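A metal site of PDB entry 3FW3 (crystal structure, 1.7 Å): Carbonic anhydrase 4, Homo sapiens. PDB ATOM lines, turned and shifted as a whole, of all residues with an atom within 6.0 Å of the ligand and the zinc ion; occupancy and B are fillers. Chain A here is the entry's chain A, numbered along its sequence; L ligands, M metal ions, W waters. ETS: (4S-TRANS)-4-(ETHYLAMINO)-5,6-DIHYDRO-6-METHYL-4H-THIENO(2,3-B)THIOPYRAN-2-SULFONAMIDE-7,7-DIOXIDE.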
ATOM      1  N   TRP A   5      -2.089   4.334  21.706  1.00  0.00           N
ATOM      2  CA  TRP A   5      -1.772   3.618  20.433  1.00  0.00           C
ATOM      3  C   TRP A   5      -0.275   3.382  20.284  1.00  0.00           C
ATOM      4  O   TRP A   5       0.538   4.152  20.780  1.00  0.00           O
ATOM      5  CB  TRP A   5      -2.319   4.400  19.203  1.00  0.00           C
ATOM      6  CG  TRP A   5      -1.603   5.693  18.822  1.00  0.00           C
ATOM      7  CD1 TRP A   5      -1.940   6.984  19.205  1.00  0.00           C
ATOM      8  CD2 TRP A   5      -0.477   5.827  17.953  1.00  0.00           C
ATOM      9  NE1 TRP A   5      -1.069   7.891  18.634  1.00  0.00           N
ATOM     10  CE2 TRP A   5      -0.161   7.197  17.861  1.00  0.00           C
ATOM     11  CE3 TRP A   5       0.315   4.906  17.251  1.00  0.00           C
ATOM     12  CZ2 TRP A   5       0.910   7.662  17.109  1.00  0.00           C
ATOM     13  CZ3 TRP A   5       1.367   5.384  16.490  1.00  0.00           C
ATOM     14  CH2 TRP A   5       1.652   6.738  16.430  1.00  0.00           C
ATOM     15  N   ASN A  68       8.855  12.650  19.898  1.00  0.00           N
ATOM     16  CA  ASN A  68       7.445  12.652  20.368  1.00  0.00           C
ATOM     17  C   ASN A  68       6.923  11.295  20.770  1.00  0.00           C
ATOM     18  O   ASN A  68       5.673  11.078  20.915  1.00  0.00           O
ATOM     19  CB  ASN A  68       6.514  13.273  19.320  1.00  0.00           C
ATOM     20  CG  ASN A  68       6.424  12.436  18.078  1.00  0.00           C
ATOM     21  OD1 ASN A  68       6.940  11.324  18.035  1.00  0.00           O
ATOM     22  ND2 ASN A  68       5.744  12.957  17.060  1.00  0.00           N
ATOM     23  N   HIS A  70       6.942   8.616  18.928  1.00  0.00           N
ATOM     24  CA  HIS A  70       6.568   7.835  17.730  1.00  0.00           C
ATOM     25  C   HIS A  70       7.585   8.015  16.585  1.00  0.00           C
ATOM     26  O   HIS A  70       7.702   7.162  15.714  1.00  0.00           O
ATOM     27  CB  HIS A  70       5.187   8.211  17.199  1.00  0.00           C
ATOM     28  CG  HIS A  70       4.136   8.366  18.259  1.00  0.00           C
ATOM     29  ND1 HIS A  70       3.803   7.371  19.146  1.00  0.00           N
ATOM     30  CD2 HIS A  70       3.344   9.428  18.578  1.00  0.00           C
ATOM     31  CE1 HIS A  70       2.877   7.807  19.974  1.00  0.00           C
ATOM     32  NE2 HIS A  70       2.570   9.045  19.645  1.00  0.00           N
ATOM     33  N   LYS A  94       4.455  22.740   8.383  1.00  0.00           N
ATOM     34  CA  LYS A  94       4.169  22.589   9.802  1.00  0.00           C
ATOM     35  C   LYS A  94       5.221  21.754  10.548  1.00  0.00           C
ATOM     36  O   LYS A  94       5.714  22.164  11.597  1.00  0.00           O
ATOM     37  CB  LYS A  94       2.791  21.975   9.981  1.00  0.00           C
ATOM     38  CG  LYS A  94       1.626  22.818   9.381  1.00  0.00           C
ATOM     39  CD  LYS A  94       1.447  24.108  10.146  1.00  0.00           C
ATOM     40  CE  LYS A  94       0.286  24.933   9.667  1.00  0.00           C
ATOM     41  NZ  LYS A  94       0.268  26.224  10.434  1.00  0.00           N
ATOM     42  N   GLN A  95       5.544  20.563  10.014  1.00  0.00           N
ATOM     43  CA  GLN A  95       6.533  19.682  10.623  1.00  0.00           C
ATOM     44  C   GLN A  95       7.144  18.715   9.621  1.00  0.00           C
ATOM     45  O   GLN A  95       6.605  18.512   8.549  1.00  0.00           O
ATOM     46  CB  GLN A  95       5.922  18.868  11.780  1.00  0.00           C
ATOM     47  CG  GLN A  95       4.772  18.041  11.362  1.00  0.00           C
ATOM     48  CD  GLN A  95       4.606  16.853  12.234  1.00  0.00           C
ATOM     49  OE1 GLN A  95       5.313  15.856  12.059  1.00  0.00           O
ATOM     50  NE2 GLN A  95       3.739  16.974  13.226  1.00  0.00           N
ATOM     51  N   HIS A  97       8.971  14.737   9.748  1.00  0.00           N
ATOM     52  CA  HIS A  97       9.313  13.598  10.574  1.00  0.00           C
ATOM     53  C   HIS A  97       9.660  12.414   9.669  1.00  0.00           C
ATOM     54  O   HIS A  97       9.512  12.492   8.453  1.00  0.00           O
ATOM     55  CB  HIS A  97       8.158  13.260  11.569  1.00  0.00           C
ATOM     56  CG  HIS A  97       6.928  12.788  10.887  1.00  0.00           C
ATOM     57  ND1 HIS A  97       5.915  13.637  10.490  1.00  0.00           N
ATOM     58  CD2 HIS A  97       6.623  11.563  10.395  1.00  0.00           C
ATOM     59  CE1 HIS A  97       5.000  12.926   9.837  1.00  0.00           C
ATOM     60  NE2 HIS A  97       5.418  11.674   9.771  1.00  0.00           N
ATOM     61  N   LEU A  98      10.086  11.300  10.280  1.00  0.00           N
ATOM     62  CA  LEU A  98      10.499  10.112   9.522  1.00  0.00           C
ATOM     63  C   LEU A  98       9.943   8.823  10.075  1.00  0.00           C
ATOM     64  O   LEU A  98       9.526   8.762  11.238  1.00  0.00           O
ATOM     65  CB  LEU A  98      12.005   9.988   9.480  1.00  0.00           C
ATOM     66  CG  LEU A  98      12.684  11.177   8.793  1.00  0.00           C
ATOM     67  CD1 LEU A  98      13.123  12.238   9.793  1.00  0.00           C
ATOM     68  CD2 LEU A  98      13.845  10.683   7.965  1.00  0.00           C
ATOM     69  N   HIS A  99       9.939   7.804   9.223  1.00  0.00           N
ATOM     70  CA  HIS A  99       9.602   6.412   9.547  1.00  0.00           C
ATOM     71  C   HIS A  99      10.798   5.570   9.084  1.00  0.00           C
ATOM     72  O   HIS A  99      11.424   5.881   8.076  1.00  0.00           O
ATOM     73  CB  HIS A  99       8.305   5.987   8.808  1.00  0.00           C
ATOM     74  CG  HIS A  99       7.126   6.874   9.099  1.00  0.00           C
ATOM     75  ND1 HIS A  99       6.234   6.615  10.119  1.00  0.00           N
ATOM     76  CD2 HIS A  99       6.693   8.010   8.497  1.00  0.00           C
ATOM     77  CE1 HIS A  99       5.327   7.593  10.154  1.00  0.00           C
ATOM     78  NE2 HIS A  99       5.588   8.444   9.184  1.00  0.00           N
ATOM     79  N   GLU A 109       6.865   3.535   4.519  1.00  0.00           N
ATOM     80  CA  GLU A 109       5.416   3.342   4.664  1.00  0.00           C
ATOM     81  C   GLU A 109       4.788   3.003   3.340  1.00  0.00           C
ATOM     82  O   GLU A 109       4.090   1.975   3.194  1.00  0.00           O
ATOM     83  CB  GLU A 109       4.750   4.559   5.344  1.00  0.00           C
ATOM     84  CG  GLU A 109       5.272   4.824   6.756  1.00  0.00           C
ATOM     85  CD  GLU A 109       4.158   5.345   7.672  1.00  0.00           C
ATOM     86  OE1 GLU A 109       3.646   6.439   7.435  1.00  0.00           O
ATOM     87  OE2 GLU A 109       3.764   4.651   8.615  1.00  0.00           O
ATOM     88  N   HIS A 122       8.563  12.520   5.775  1.00  0.00           N
ATOM     89  CA  HIS A 122       7.267  13.126   5.577  1.00  0.00           C
ATOM     90  C   HIS A 122       7.355  14.616   5.924  1.00  0.00           C
ATOM     91  O   HIS A 122       7.644  14.973   7.075  1.00  0.00           O
ATOM     92  CB  HIS A 122       6.237  12.448   6.471  1.00  0.00           C
ATOM     93  CG  HIS A 122       5.806  11.107   5.968  1.00  0.00           C
ATOM     94  ND1 HIS A 122       4.999  10.256   6.684  1.00  0.00           N
ATOM     95  CD2 HIS A 122       6.164  10.421   4.852  1.00  0.00           C
ATOM     96  CE1 HIS A 122       4.799   9.145   5.995  1.00  0.00           C
ATOM     97  NE2 HIS A 122       5.493   9.223   4.868  1.00  0.00           N
ATOM     98  N   VAL A 124       5.124  17.739   6.304  1.00  0.00           N
ATOM     99  CA  VAL A 124       3.698  17.948   6.520  1.00  0.00           C
ATOM    100  C   VAL A 124       3.332  19.441   6.419  1.00  0.00           C
ATOM    101  O   VAL A 124       3.948  20.270   7.074  1.00  0.00           O
ATOM    102  CB  VAL A 124       3.266  17.441   7.893  1.00  0.00           C
ATOM    103  CG1 VAL A 124       1.744  17.621   8.094  1.00  0.00           C
ATOM    104  CG2 VAL A 124       3.712  15.982   8.119  1.00  0.00           C
ATOM    105  N   ILE A 145      -4.452  18.666   4.412  1.00  0.00           N
ATOM    106  CA  ILE A 145      -3.044  18.460   4.647  1.00  0.00           C
ATOM    107  C   ILE A 145      -2.373  17.923   3.373  1.00  0.00           C
ATOM    108  O   ILE A 145      -2.908  17.024   2.706  1.00  0.00           O
ATOM    109  CB  ILE A 145      -2.856  17.490   5.829  1.00  0.00           C
ATOM    110  CG1 ILE A 145      -3.370  18.149   7.123  1.00  0.00           C
ATOM    111  CG2 ILE A 145      -1.389  17.062   5.965  1.00  0.00           C
ATOM    112  CD1 ILE A 145      -3.436  17.259   8.285  1.00  0.00           C
ATOM    113  N   VAL A 147       1.103  16.115   2.426  1.00  0.00           N
ATOM    114  CA  VAL A 147       2.362  15.539   2.836  1.00  0.00           C
ATOM    115  C   VAL A 147       3.229  15.262   1.618  1.00  0.00           C
ATOM    116  O   VAL A 147       2.779  14.587   0.661  1.00  0.00           O
ATOM    117  CB  VAL A 147       2.165  14.193   3.663  1.00  0.00           C
ATOM    118  CG1 VAL A 147       3.538  13.634   4.097  1.00  0.00           C
ATOM    119  CG2 VAL A 147       1.301  14.420   4.883  1.00  0.00           C
ATOM    120  N   SER A 205      -4.999   9.337   3.868  1.00  0.00           N
ATOM    121  CA  SER A 205      -5.110   9.618   5.290  1.00  0.00           C
ATOM    122  C   SER A 205      -3.802   9.900   5.991  1.00  0.00           C
ATOM    123  O   SER A 205      -2.717   9.654   5.462  1.00  0.00           O
ATOM    124  CB  SER A 205      -5.799   8.430   5.977  1.00  0.00           C
ATOM    125  OG  SER A 205      -4.871   7.346   6.243  1.00  0.00           O
ATOM    126  N   LEU A 206      -3.920  10.359   7.230  1.00  0.00           N
ATOM    127  CA  LEU A 206      -2.811  10.337   8.147  1.00  0.00           C
ATOM    128  C   LEU A 206      -2.464   8.871   8.419  1.00  0.00           C
ATOM    129  O   LEU A 206      -3.377   8.005   8.430  1.00  0.00           O
ATOM    130  CB  LEU A 206      -3.174  10.989   9.454  1.00  0.00           C
ATOM    131  CG  LEU A 206      -3.550  12.464   9.394  1.00  0.00           C
ATOM    132  CD1 LEU A 206      -3.956  12.892  10.798  1.00  0.00           C
ATOM    133  CD2 LEU A 206      -2.401  13.300   8.901  1.00  0.00           C
ATOM    134  N   THR A 207      -1.194   8.559   8.563  1.00  0.00           N
ATOM    135  CA  THR A 207      -0.739   7.150   8.838  1.00  0.00           C
ATOM    136  C   THR A 207      -0.634   6.782  10.342  1.00  0.00           C
ATOM    137  O   THR A 207      -0.068   5.755  10.685  1.00  0.00           O
ATOM    138  CB  THR A 207       0.576   6.801   8.129  1.00  0.00           C
ATOM    139  OG1 THR A 207       1.635   7.563   8.704  1.00  0.00           O
ATOM    140  CG2 THR A 207       0.500   7.146   6.665  1.00  0.00           C
ATOM    141  N   THR A 208      -1.111   7.658  11.200  1.00  0.00           N
ATOM    142  CA  THR A 208      -1.228   7.387  12.653  1.00  0.00           C
ATOM    143  C   THR A 208      -2.634   7.770  13.085  1.00  0.00           C
ATOM    144  O   THR A 208      -3.287   8.538  12.401  1.00  0.00           O
ATOM    145  CB  THR A 208      -0.211   8.201  13.499  1.00  0.00           C
ATOM    146  OG1 THR A 208      -0.496   9.614  13.395  1.00  0.00           O
ATOM    147  CG2 THR A 208       1.204   8.087  13.001  1.00  0.00           C
ATOM    148  N   PRO A 209      -3.117   7.263  14.230  1.00  0.00           N
ATOM    149  CA  PRO A 209      -4.385   7.734  14.774  1.00  0.00           C
ATOM    150  C   PRO A 209      -4.342   9.273  14.872  1.00  0.00           C
ATOM    151  O   PRO A 209      -3.287   9.787  15.161  1.00  0.00           O
ATOM    152  CB  PRO A 209      -4.421   7.078  16.160  1.00  0.00           C
ATOM    153  CG  PRO A 209      -3.732   5.799  15.921  1.00  0.00           C
ATOM    154  CD  PRO A 209      -2.543   6.197  15.073  1.00  0.00           C
ATOM    155  N   LYS A 214      -7.890  13.228   5.146  1.00  0.00           N
ATOM    156  CA  LYS A 214      -7.770  14.666   4.802  1.00  0.00           C
ATOM    157  C   LYS A 214      -6.410  15.040   4.217  1.00  0.00           C
ATOM    158  O   LYS A 214      -6.047  16.213   4.147  1.00  0.00           O
ATOM    159  CB  LYS A 214      -8.069  15.549   6.011  1.00  0.00           C
ATOM    160  CG  LYS A 214      -7.076  15.397   7.147  1.00  0.00           C
ATOM    161  CD  LYS A 214      -7.642  16.052   8.434  1.00  0.00           C
ATOM    162  CE  LYS A 214      -6.611  16.046   9.565  1.00  0.00           C
ATOM    163  NZ  LYS A 214      -7.008  16.890  10.740  1.00  0.00           N
ATOM    164  N   VAL A 215      -5.700  14.034   3.711  1.00  0.00           N
ATOM    165  CA  VAL A 215      -4.359  14.221   3.211  1.00  0.00           C
ATOM    166  C   VAL A 215      -4.309  14.055   1.680  1.00  0.00           C
ATOM    167  O   VAL A 215      -4.771  13.059   1.111  1.00  0.00           O
ATOM    168  CB  VAL A 215      -3.340  13.236   3.851  1.00  0.00           C
ATOM    169  CG1 VAL A 215      -1.932  13.504   3.287  1.00  0.00           C
ATOM    170  CG2 VAL A 215      -3.368  13.348   5.353  1.00  0.00           C
ATOM    171  N   TRP A 217      -1.595  13.189  -0.780  1.00  0.00           N
ATOM    172  CA  TRP A 217      -0.255  12.612  -0.784  1.00  0.00           C
ATOM    173  C   TRP A 217       0.532  12.847  -2.059  1.00  0.00           C
ATOM    174  O   TRP A 217      -0.014  12.836  -3.133  1.00  0.00           O
ATOM    175  CB  TRP A 217      -0.330  11.085  -0.551  1.00  0.00           C
ATOM    176  CG  TRP A 217      -0.536  10.754   0.888  1.00  0.00           C
ATOM    177  CD1 TRP A 217      -1.726  10.521   1.501  1.00  0.00           C
ATOM    178  CD2 TRP A 217       0.452  10.690   1.922  1.00  0.00           C
ATOM    179  NE1 TRP A 217      -1.553  10.282   2.829  1.00  0.00           N
ATOM    180  CE2 TRP A 217      -0.230  10.340   3.134  1.00  0.00           C
ATOM    181  CE3 TRP A 217       1.842  10.824   1.962  1.00  0.00           C
ATOM    182  CZ2 TRP A 217       0.428  10.220   4.366  1.00  0.00           C
ATOM    183  CZ3 TRP A 217       2.498  10.623   3.145  1.00  0.00           C
ATOM    184  CH2 TRP A 217       1.785  10.347   4.357  1.00  0.00           C
HETATM  185  S1  ETS L   1       1.159  13.975   9.715  1.00  0.00           S
HETATM  186  C2  ETS L   1       1.266  12.223   9.914  1.00  0.00           C
HETATM  187  C3  ETS L   1       0.850  11.964  11.191  1.00  0.00           C
HETATM  188  C4  ETS L   1       0.437  13.071  11.961  1.00  0.00           C
HETATM  189  C5  ETS L   1      -0.165  12.979  13.364  1.00  0.00           C
HETATM  190  C6  ETS L   1      -1.038  14.202  13.694  1.00  0.00           C
HETATM  191  C7  ETS L   1      -0.293  15.549  13.571  1.00  0.00           C
HETATM  192  S8  ETS L   1      -0.001  15.873  11.828  1.00  0.00           S
HETATM  193  C9  ETS L   1       0.495  14.278  11.314  1.00  0.00           C
HETATM  194  S10 ETS L   1       1.745  11.314   8.526  1.00  0.00           S
HETATM  195  O11 ETS L   1       2.597  12.209   7.786  1.00  0.00           O
HETATM  196  O12 ETS L   1       0.528  10.813   7.964  1.00  0.00           O
HETATM  197  N13 ETS L   1       2.551  10.011   9.122  1.00  0.00           N
HETATM  198  N14 ETS L   1       0.919  12.882  14.354  1.00  0.00           N
HETATM  199  C15 ETS L   1      -1.132  16.732  14.080  1.00  0.00           C
HETATM  200  O16 ETS L   1      -1.233  16.026  11.175  1.00  0.00           O
HETATM  201  O17 ETS L   1       1.099  16.719  11.558  1.00  0.00           O
HETATM  202  C18 ETS L   1       1.345  11.505  14.580  1.00  0.00           C
HETATM  203  C19 ETS L   1       2.253  11.456  15.808  1.00  0.00           C
HETATM  204 ZN    ZN M   1       4.538  10.172   8.701  1.00  0.00          ZN
HETATM  205  O   HOH W   1       4.456  11.352  13.129  1.00  0.00           O
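N of Thr 207 lies within hydrogen-bond range of O12 of the ligand.
OG1 of Thr 207 sits close to N13 of the ligand (2.6 Å).
O17 of the ligand sits at hydrogen-bond distance from NE2 of Gln 95 (3.1 Å).
The side-chain hydroxyl (OG1) of Thr 207 lies within hydrogen-bond range of the side-chain carboxylate (OE1) of Glu 109 (2.6 Å).
ND1 of His 97 lies within hydrogen-bond range of OE1 of Gln 95 (2.8 Å).
A ring nitrogen (ND1) of His 99 sits close to the side-chain carboxylate of Glu 109 (3.5 Å).
The backbone carbonyl oxygen (O) of Gln 95 sits at hydrogen-bond distance from the backbone NH (N) of Val 124 (2.8 Å).
NE1 of Trp 217 lies within hydrogen-bond range of O of Ser 205, 2.9 Å away.
O of Val 124 lies within hydrogen-bond range of N of Lys 94, 2.8 Å away.
The backbone NH (N) of His 70 lies within hydrogen-bond range of the side-chain amide oxygen (OD1) of Asn 68, at 2.9 Å.
The backbone NH (N) of Ile 145 is in hydrogen-bond range of the backbone carbonyl oxygen (O) of Lys 214.
Residues that only touch the ligand: Thr 208 (2.9 Å), Leu 206 (3.4 Å), His 70 (3.6 Å), Val 124 (3.6 Å), Trp 217 (3.6 Å), Ile 145 (3.8 Å) and Val 147 (3.9 Å).
Merely in contact with the zinc ion: Thr 207 (3.9 Å).
Four residues have an atom within 4 Å of the zinc ion: His 97, His 99, His 122 and Thr 207.
Along chain A the residues within 4 Å of the zinc ion span positions 97 to 207.
The nearest printed residue that does not touch the zinc ion is Glu 109 (4.04 Å).
The zinc ion is bound by N13 of the ligand (2.0 Å), NE2 of His 97 (2.0 Å), ND1 of His 122 (2.1 Å) and NE2 of His 99 (2.1 Å).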
